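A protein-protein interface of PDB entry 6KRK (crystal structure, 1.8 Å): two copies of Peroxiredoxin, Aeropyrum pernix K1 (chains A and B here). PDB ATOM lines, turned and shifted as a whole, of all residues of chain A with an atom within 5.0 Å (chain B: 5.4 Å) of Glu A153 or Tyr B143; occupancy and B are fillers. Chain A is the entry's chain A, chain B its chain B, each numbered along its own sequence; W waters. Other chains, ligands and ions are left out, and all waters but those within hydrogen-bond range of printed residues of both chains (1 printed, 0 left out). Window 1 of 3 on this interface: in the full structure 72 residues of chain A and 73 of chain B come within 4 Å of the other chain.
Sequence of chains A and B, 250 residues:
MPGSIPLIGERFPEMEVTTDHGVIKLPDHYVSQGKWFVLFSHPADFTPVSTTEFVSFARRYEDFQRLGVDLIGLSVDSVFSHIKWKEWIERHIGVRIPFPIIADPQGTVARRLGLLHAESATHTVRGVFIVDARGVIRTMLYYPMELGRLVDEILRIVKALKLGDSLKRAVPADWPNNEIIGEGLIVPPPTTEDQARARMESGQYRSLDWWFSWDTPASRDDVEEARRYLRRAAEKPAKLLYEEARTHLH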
ATOM      1  N   ILE A   8     -15.622  10.602  11.788  1.00  0.00           N
ATOM      2  CA  ILE A   8     -16.836  10.438  10.950  1.00  0.00           C
ATOM      3  C   ILE A   8     -16.404  10.086   9.520  1.00  0.00           C
ATOM      4  O   ILE A   8     -15.481  10.736   9.010  1.00  0.00           O
ATOM      5  CB  ILE A   8     -17.690  11.705  11.008  1.00  0.00           C
ATOM      6  CG1 ILE A   8     -18.326  11.853  12.393  1.00  0.00           C
ATOM      7  CG2 ILE A   8     -18.763  11.653   9.935  1.00  0.00           C
ATOM      8  CD1 ILE A   8     -18.944  13.230  12.587  1.00  0.00           C
ATOM      9  N   THR A 139     -21.709   9.648  13.392  1.00  0.00           N
ATOM     10  CA  THR A 139     -21.824  10.777  14.363  1.00  0.00           C
ATOM     11  C   THR A 139     -21.058  10.376  15.612  1.00  0.00           C
ATOM     12  O   THR A 139     -21.134   9.207  15.991  1.00  0.00           O
ATOM     13  CB  THR A 139     -23.308  11.086  14.615  1.00  0.00           C
ATOM     14  OG1 THR A 139     -23.914  11.695  13.472  1.00  0.00           O
ATOM     15  CG2 THR A 139     -23.537  12.036  15.768  1.00  0.00           C
ATOM     16  N   MET A 140     -20.456  11.344  16.309  1.00  0.00           N
ATOM     17  CA  MET A 140     -19.804  11.078  17.609  1.00  0.00           C
ATOM     18  C   MET A 140     -20.191  12.193  18.577  1.00  0.00           C
ATOM     19  O   MET A 140     -20.163  13.368  18.196  1.00  0.00           O
ATOM     20  CB  MET A 140     -18.292  11.044  17.447  1.00  0.00           C
ATOM     21  CG  MET A 140     -17.876   9.995  16.460  1.00  0.00           C
ATOM     22  SD  MET A 140     -16.070  10.014  16.287  1.00  0.00           S
ATOM     23  CE  MET A 140     -15.859  11.410  15.226  1.00  0.00           C
ATOM     24  N   LEU A 141     -20.517  11.813  19.798  1.00  0.00           N
ATOM     25  CA  LEU A 141     -20.879  12.791  20.850  1.00  0.00           C
ATOM     26  C   LEU A 141     -20.007  12.492  22.054  1.00  0.00           C
ATOM     27  O   LEU A 141     -19.807  11.311  22.358  1.00  0.00           O
ATOM     28  CB  LEU A 141     -22.336  12.649  21.259  1.00  0.00           C
ATOM     29  CG  LEU A 141     -23.344  12.519  20.127  1.00  0.00           C
ATOM     30  CD1 LEU A 141     -24.693  12.146  20.721  1.00  0.00           C
ATOM     31  CD2 LEU A 141     -23.393  13.826  19.379  1.00  0.00           C
ATOM     32  N   LEU A 150     -29.188  12.989  26.382  1.00  0.00           N
ATOM     33  CA  LEU A 150     -30.606  13.066  25.970  1.00  0.00           C
ATOM     34  C   LEU A 150     -30.809  11.920  24.989  1.00  0.00           C
ATOM     35  O   LEU A 150     -30.445  12.062  23.801  1.00  0.00           O
ATOM     36  CB  LEU A 150     -30.850  14.432  25.334  1.00  0.00           C
ATOM     37  CG  LEU A 150     -32.305  14.707  24.992  1.00  0.00           C
ATOM     38  CD1 LEU A 150     -33.102  14.969  26.270  1.00  0.00           C
ATOM     39  CD2 LEU A 150     -32.437  15.864  24.028  1.00  0.00           C
ATOM     40  N   VAL A 151     -31.297  10.780  25.454  1.00  0.00           N
ATOM     41  CA  VAL A 151     -31.326   9.579  24.579  1.00  0.00           C
ATOM     42  C   VAL A 151     -32.227   9.786  23.350  1.00  0.00           C
ATOM     43  O   VAL A 151     -31.930   9.180  22.278  1.00  0.00           O
ATOM     44  CB  VAL A 151     -31.655   8.345  25.414  1.00  0.00           C
ATOM     45  CG1 VAL A 151     -31.712   7.096  24.564  1.00  0.00           C
ATOM     46  CG2 VAL A 151     -30.638   8.196  26.542  1.00  0.00           C
ATOM     47  N   ASP A 152     -33.272  10.604  23.447  1.00  0.00           N
ATOM     48  CA  ASP A 152     -34.203  10.849  22.306  1.00  0.00           C
ATOM     49  C   ASP A 152     -33.453  11.533  21.147  1.00  0.00           C
ATOM     50  O   ASP A 152     -33.840  11.323  20.012  1.00  0.00           O
ATOM     51  CB  ASP A 152     -35.451  11.603  22.778  1.00  0.00           C
ATOM     52  CG  ASP A 152     -36.358  10.702  23.632  1.00  0.00           C
ATOM     53  OD1 ASP A 152     -36.631   9.578  23.220  1.00  0.00           O
ATOM     54  OD2 ASP A 152     -36.716  11.097  24.730  1.00  0.00           O
ATOM     55  N   GLU A 153     -32.403  12.325  21.415  1.00  0.00           N
ATOM     56  CA  GLU A 153     -31.622  12.949  20.302  1.00  0.00           C
ATOM     57  C   GLU A 153     -30.850  11.862  19.560  1.00  0.00           C
ATOM     58  O   GLU A 153     -30.700  11.996  18.336  1.00  0.00           O
ATOM     59  CB  GLU A 153     -30.694  14.047  20.800  1.00  0.00           C
ATOM     60  CG  GLU A 153     -29.761  14.624  19.730  1.00  0.00           C
ATOM     61  CD  GLU A 153     -30.428  15.189  18.484  1.00  0.00           C
ATOM     62  OE1 GLU A 153     -31.665  15.110  18.362  1.00  0.00           O
ATOM     63  OE2 GLU A 153     -29.708  15.693  17.610  1.00  0.00           O
ATOM     64  N   ILE A 154     -30.375  10.812  20.246  1.00  0.00           N
ATOM     65  CA  ILE A 154     -29.678   9.671  19.601  1.00  0.00           C
ATOM     66  C   ILE A 154     -30.645   8.953  18.653  1.00  0.00           C
ATOM     67  O   ILE A 154     -30.326   8.729  17.471  1.00  0.00           O
ATOM     68  CB  ILE A 154     -29.044   8.720  20.633  1.00  0.00           C
ATOM     69  CG1 ILE A 154     -28.017   9.446  21.494  1.00  0.00           C
ATOM     70  CG2 ILE A 154     -28.437   7.511  19.934  1.00  0.00           C
ATOM     71  CD1 ILE A 154     -27.427   8.580  22.628  1.00  0.00           C
ATOM     72  N   LEU A 155     -31.889   8.748  19.069  1.00  0.00           N
ATOM     73  CA  LEU A 155     -32.900   8.180  18.143  1.00  0.00           C
ATOM     74  C   LEU A 155     -33.167   9.106  16.946  1.00  0.00           C
ATOM     75  O   LEU A 155     -33.302   8.591  15.848  1.00  0.00           O
ATOM     76  CB  LEU A 155     -34.189   7.975  18.922  1.00  0.00           C
ATOM     77  CG  LEU A 155     -34.175   6.790  19.883  1.00  0.00           C
ATOM     78  CD1 LEU A 155     -35.385   6.855  20.820  1.00  0.00           C
ATOM     79  CD2 LEU A 155     -34.218   5.498  19.087  1.00  0.00           C
ATOM     80  N   ARG A 156     -33.295  10.398  17.170  1.00  0.00           N
ATOM     81  CA  ARG A 156     -33.590  11.385  16.091  1.00  0.00           C
ATOM     82  C   ARG A 156     -32.435  11.336  15.085  1.00  0.00           C
ATOM     83  O   ARG A 156     -32.712  11.304  13.910  1.00  0.00           O
ATOM     84  CB  ARG A 156     -33.779  12.796  16.639  1.00  0.00           C
ATOM     85  CG  ARG A 156     -34.266  13.820  15.598  1.00  0.00           C
ATOM     86  CD  ARG A 156     -34.122  15.261  16.042  1.00  0.00           C
ATOM     87  NE  ARG A 156     -32.721  15.671  15.982  1.00  0.00           N
ATOM     88  CZ  ARG A 156     -32.131  16.296  14.968  1.00  0.00           C
ATOM     89  NH1 ARG A 156     -32.818  16.640  13.889  1.00  0.00           N
ATOM     90  NH2 ARG A 156     -30.823  16.536  15.005  1.00  0.00           N
ATOM     91  N   ILE A 157     -31.195  11.346  15.552  1.00  0.00           N
ATOM     92  CA  ILE A 157     -29.995  11.235  14.678  1.00  0.00           C
ATOM     93  C   ILE A 157     -30.114  10.001  13.783  1.00  0.00           C
ATOM     94  O   ILE A 157     -29.961  10.155  12.553  1.00  0.00           O
ATOM     95  CB  ILE A 157     -28.708  11.224  15.527  1.00  0.00           C
ATOM     96  CG1 ILE A 157     -28.480  12.609  16.122  1.00  0.00           C
ATOM     97  CG2 ILE A 157     -27.529  10.754  14.695  1.00  0.00           C
ATOM     98  CD1 ILE A 157     -27.546  12.650  17.304  1.00  0.00           C
ATOM     99  N   LEU A 230     -38.894  13.651  20.161  1.00  0.00           N
ATOM    100  CA  LEU A 230     -38.671  14.968  20.796  1.00  0.00           C
ATOM    101  C   LEU A 230     -39.822  15.277  21.754  1.00  0.00           C
ATOM    102  O   LEU A 230     -39.529  15.900  22.785  1.00  0.00           O
ATOM    103  CB  LEU A 230     -38.527  16.032  19.719  1.00  0.00           C
ATOM    104  CG  LEU A 230     -37.351  15.834  18.758  1.00  0.00           C
ATOM    105  CD1 LEU A 230     -37.472  16.833  17.629  1.00  0.00           C
ATOM    106  CD2 LEU A 230     -36.027  15.966  19.492  1.00  0.00           C
ATOM    107  N   VAL B 125     -16.459  19.086   9.508  1.00  0.00           N
ATOM    108  CA  VAL B 125     -17.790  18.577   9.918  1.00  0.00           C
ATOM    109  C   VAL B 125     -18.445  19.612  10.845  1.00  0.00           C
ATOM    110  O   VAL B 125     -17.967  20.760  11.005  1.00  0.00           O
ATOM    111  CB  VAL B 125     -17.680  17.174  10.553  1.00  0.00           C
ATOM    112  CG1 VAL B 125     -17.290  16.115   9.508  1.00  0.00           C
ATOM    113  CG2 VAL B 125     -16.720  17.159  11.718  1.00  0.00           C
ATOM    114  N   ARG B 126     -19.550  19.205  11.443  1.00  0.00           N
ATOM    115  CA  ARG B 126     -20.411  20.092  12.269  1.00  0.00           C
ATOM    116  C   ARG B 126     -20.023  19.845  13.703  1.00  0.00           C
ATOM    117  O   ARG B 126     -20.779  19.189  14.421  1.00  0.00           O
ATOM    118  CB  ARG B 126     -21.875  19.757  11.972  1.00  0.00           C
ATOM    119  CG  ARG B 126     -22.289  20.052  10.537  1.00  0.00           C
ATOM    120  CD  ARG B 126     -23.809  19.906  10.288  1.00  0.00           C
ATOM    121  NE  ARG B 126     -23.988  19.824   8.858  1.00  0.00           N
ATOM    122  CZ  ARG B 126     -23.955  20.875   8.030  1.00  0.00           C
ATOM    123  NH1 ARG B 126     -23.904  20.662   6.737  1.00  0.00           N
ATOM    124  NH2 ARG B 126     -23.881  22.119   8.492  1.00  0.00           N
ATOM    125  N   GLY B 127     -18.878  20.381  14.096  1.00  0.00           N
ATOM    126  CA  GLY B 127     -18.360  20.240  15.446  1.00  0.00           C
ATOM    127  C   GLY B 127     -18.987  21.260  16.359  1.00  0.00           C
ATOM    128  O   GLY B 127     -19.443  22.324  15.895  1.00  0.00           O
ATOM    129  N   LEU B 141     -19.507  17.794  20.518  1.00  0.00           N
ATOM    130  CA  LEU B 141     -20.375  17.020  19.618  1.00  0.00           C
ATOM    131  C   LEU B 141     -19.775  17.078  18.213  1.00  0.00           C
ATOM    132  O   LEU B 141     -19.338  18.163  17.781  1.00  0.00           O
ATOM    133  CB  LEU B 141     -21.759  17.658  19.604  1.00  0.00           C
ATOM    134  CG  LEU B 141     -22.361  18.063  20.958  1.00  0.00           C
ATOM    135  CD1 LEU B 141     -23.667  18.801  20.733  1.00  0.00           C
ATOM    136  CD2 LEU B 141     -22.573  16.827  21.846  1.00  0.00           C
ATOM    137  N   TYR B 142     -19.868  15.990  17.478  1.00  0.00           N
ATOM    138  CA  TYR B 142     -19.444  15.953  16.058  1.00  0.00           C
ATOM    139  C   TYR B 142     -20.591  15.379  15.228  1.00  0.00           C
ATOM    140  O   TYR B 142     -20.813  14.186  15.228  1.00  0.00           O
ATOM    141  CB  TYR B 142     -18.175  15.112  15.914  1.00  0.00           C
ATOM    142  CG  TYR B 142     -16.967  15.698  16.609  1.00  0.00           C
ATOM    143  CD1 TYR B 142     -16.160  16.647  15.992  1.00  0.00           C
ATOM    144  CD2 TYR B 142     -16.644  15.312  17.889  1.00  0.00           C
ATOM    145  CE1 TYR B 142     -15.045  17.170  16.630  1.00  0.00           C
ATOM    146  CE2 TYR B 142     -15.548  15.846  18.558  1.00  0.00           C
ATOM    147  CZ  TYR B 142     -14.722  16.741  17.907  1.00  0.00           C
ATOM    148  OH  TYR B 142     -13.642  17.281  18.544  1.00  0.00           O
ATOM    149  N   TYR B 143     -21.366  16.274  14.640  1.00  0.00           N
ATOM    150  CA  TYR B 143     -22.392  15.947  13.646  1.00  0.00           C
ATOM    151  C   TYR B 143     -21.756  15.945  12.256  1.00  0.00           C
ATOM    152  O   TYR B 143     -20.720  16.567  12.006  1.00  0.00           O
ATOM    153  CB  TYR B 143     -23.530  16.950  13.729  1.00  0.00           C
ATOM    154  CG  TYR B 143     -24.481  16.712  14.876  1.00  0.00           C
ATOM    155  CD1 TYR B 143     -24.069  16.832  16.201  1.00  0.00           C
ATOM    156  CD2 TYR B 143     -25.815  16.400  14.643  1.00  0.00           C
ATOM    157  CE1 TYR B 143     -24.960  16.664  17.258  1.00  0.00           C
ATOM    158  CE2 TYR B 143     -26.698  16.190  15.700  1.00  0.00           C
ATOM    159  CZ  TYR B 143     -26.266  16.285  17.013  1.00  0.00           C
ATOM    160  OH  TYR B 143     -27.182  16.190  18.049  1.00  0.00           O
ATOM    161  N   PRO B 144     -22.344  15.193  11.318  1.00  0.00           N
ATOM    162  CA  PRO B 144     -21.792  15.036   9.975  1.00  0.00           C
ATOM    163  C   PRO B 144     -22.366  16.067   9.000  1.00  0.00           C
ATOM    164  O   PRO B 144     -23.288  16.788   9.320  1.00  0.00           O
ATOM    165  CB  PRO B 144     -22.282  13.623   9.618  1.00  0.00           C
ATOM    166  CG  PRO B 144     -23.652  13.541  10.245  1.00  0.00           C
ATOM    167  CD  PRO B 144     -23.561  14.404  11.507  1.00  0.00           C
ATOM    168  N   MET B 145     -21.870  16.069   7.765  1.00  0.00           N
ATOM    169  CA  MET B 145     -22.286  17.055   6.748  1.00  0.00           C
ATOM    170  C   MET B 145     -23.793  16.955   6.505  1.00  0.00           C
ATOM    171  O   MET B 145     -24.440  18.007   6.292  1.00  0.00           O
ATOM    172  CB  MET B 145     -21.574  16.794   5.419  1.00  0.00           C
ATOM    173  CG  MET B 145     -20.080  16.744   5.521  1.00  0.00           C
ATOM    174  SD  MET B 145     -19.482  18.203   6.342  1.00  0.00           S
ATOM    175  CE  MET B 145     -17.751  17.953   5.937  1.00  0.00           C
ATOM    176  N   LEU B 147     -26.458  16.137   8.249  1.00  0.00           N
ATOM    177  CA  LEU B 147     -27.447  16.156   9.379  1.00  0.00           C
ATOM    178  C   LEU B 147     -27.241  17.435  10.190  1.00  0.00           C
ATOM    179  O   LEU B 147     -26.200  17.529  10.854  1.00  0.00           O
ATOM    180  CB  LEU B 147     -27.158  14.963  10.269  1.00  0.00           C
ATOM    181  CG  LEU B 147     -28.250  14.320  11.128  1.00  0.00           C
ATOM    182  CD1 LEU B 147     -27.726  13.864  12.480  1.00  0.00           C
ATOM    183  CD2 LEU B 147     -29.612  14.957  11.138  1.00  0.00           C
ATOM    184  N   GLY B 148     -28.213  18.318  10.187  1.00  0.00           N
ATOM    185  CA  GLY B 148     -28.269  19.507  11.052  1.00  0.00           C
ATOM    186  C   GLY B 148     -28.359  19.165  12.525  1.00  0.00           C
ATOM    187  O   GLY B 148     -28.973  18.132  12.891  1.00  0.00           O
ATOM    188  N   ARG B 149     -27.803  20.041  13.344  1.00  0.00           N
ATOM    189  CA  ARG B 149     -27.821  19.884  14.823  1.00  0.00           C
ATOM    190  C   ARG B 149     -29.227  20.217  15.368  1.00  0.00           C
ATOM    191  O   ARG B 149     -30.103  20.747  14.631  1.00  0.00           O
ATOM    192  CB  ARG B 149     -26.709  20.740  15.439  1.00  0.00           C
ATOM    193  CG  ARG B 149     -25.341  20.150  15.153  1.00  0.00           C
ATOM    194  CD  ARG B 149     -24.164  21.101  15.269  1.00  0.00           C
ATOM    195  NE  ARG B 149     -24.073  21.902  14.060  1.00  0.00           N
ATOM    196  CZ  ARG B 149     -22.979  22.530  13.647  1.00  0.00           C
ATOM    197  NH1 ARG B 149     -21.868  22.474  14.364  1.00  0.00           N
ATOM    198  NH2 ARG B 149     -22.996  23.176  12.489  1.00  0.00           N
ATOM    199  N   LEU B 150     -29.439  19.768  16.592  1.00  0.00           N
ATOM    200  CA  LEU B 150     -30.665  20.047  17.390  1.00  0.00           C
ATOM    201  C   LEU B 150     -30.246  21.135  18.365  1.00  0.00           C
ATOM    202  O   LEU B 150     -29.567  20.820  19.350  1.00  0.00           O
ATOM    203  CB  LEU B 150     -31.127  18.791  18.132  1.00  0.00           C
ATOM    204  CG  LEU B 150     -32.467  18.976  18.859  1.00  0.00           C
ATOM    205  CD1 LEU B 150     -33.593  18.975  17.834  1.00  0.00           C
ATOM    206  CD2 LEU B 150     -32.697  17.916  19.925  1.00  0.00           C
ATOM    207  N   GLU B 153     -30.789  21.127  22.167  1.00  0.00           N
ATOM    208  CA  GLU B 153     -30.008  20.221  23.066  1.00  0.00           C
ATOM    209  C   GLU B 153     -28.752  20.965  23.523  1.00  0.00           C
ATOM    210  O   GLU B 153     -28.260  20.702  24.622  1.00  0.00           O
ATOM    211  CB  GLU B 153     -29.655  18.898  22.395  1.00  0.00           C
ATOM    212  CG  GLU B 153     -28.601  18.070  23.160  1.00  0.00           C
ATOM    213  CD  GLU B 153     -28.986  17.654  24.573  1.00  0.00           C
ATOM    214  OE1 GLU B 153     -30.098  18.070  24.996  1.00  0.00           O
ATOM    215  OE2 GLU B 153     -28.231  16.857  25.242  1.00  0.00           O
HETATM  216  O   HOH W   1     -31.336  17.651  11.817  1.00  0.00           O
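OH of Tyr B143 lies within hydrogen-bond range of OE2 of Glu A153.
NH2 of Arg A156 lies within hydrogen-bond range of O of Gly B148.
O of Met A140 is in hydrogen-bond range of N of Tyr B142, 2.7 Å away.
N of Arg B126 sits at hydrogen-bond distance from O of Tyr B143, 2.9 Å away.
NE of Arg B126 is in hydrogen-bond range of O of Pro B144, at 3.1 Å.
The side-chain carboxylate (OE1) of Glu A153 lies within salt-bridge range of the guanidinium group (NE) of Arg A156 (2.7 Å).
Tyr B142 touches Ile A8.
Pro B144 touches Thr A139 (CD to OG1, 3.4 Å).
Met A140 touches Leu B141.
Leu A141 touches Leu B141 (CD2 to CD2, 3.97 Å).
Tyr B143 touches Leu A141 (CE1 to CD2, 3.9 Å).
Glu B153 touches Leu A150.
Leu B150 touches Arg A156 (N to NH2, 3.9 Å).
Ile A157 touches Tyr B143 (CD1 to OH, 3.6 Å).
CD1 of Leu B147 touches CG2 of Ile A157, at 3.8 Å.
CD2 of Leu B150 touches CD2 of Leu A230, at 3.9 Å.
Printed residues of chain B within 4 Å of Ile A8: Tyr B142 and Tyr B143.
Glu A153 touches just these residues of chain B: Tyr B143 and Leu B150.
Printed residues of chain B within 4 Å of Arg A156: Gly B148 (3.2 Å) and Leu B150 (3.9 Å).
Val B125 touches none of the printed residues of chain A.
Tyr B143 touches just these residues of chain A: Ile A8 (3.8 Å), Leu A141 (3.9 Å), Glu A153 (2.6 Å) and Ile A157 (3.6 Å).
Of the printed residues of chain A, Leu B147 touches Ile A157 (3.8 Å).
The nearest residue of chain A that does not touch Tyr B143 is Arg A156 (4.2 Å).
Hydrophobic or aromatic side chains of chain A that line the printed part of chain B: Ile A8, Leu A141, Leu A150, Ile A157 and Leu A230.
Of the 13 printed residues of chain B, 8 touch a printed residue of chain A.
Printed residues of chain B that touch a printed residue of chain A: Leu B141, Tyr B142, Tyr B143, Pro B144, Leu B147, Gly B148, Leu B150 and Glu B153.
Hydrophobic or aromatic side chains of chain B that line the printed part of chain A: Leu B141, Tyr B142, Tyr B143, Pro B144, Leu B147 and Leu B150.
Among the printed residues, 16 pairs touch across the chains.
Among the printed residues, no Asp or Glu carboxylate lies within 4 Å of a Lys or Arg side-chain nitrogen of the other chain.
Leu B141 touches its own counterpart, Leu A141.
Leu A150 touches Glu B153, and with the chains exchanged Glu A153 touches Leu B150.
Of the 16 pairs that touch across the chains among the printed residues, 3 have their exchanged pair printed and touching as well.
Water W1 lies within hydrogen-bond range of the backbone carbonyl oxygen of Gly B148 (2.6 Å) and the guanidinium group of Arg A156 (2.7 Å).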
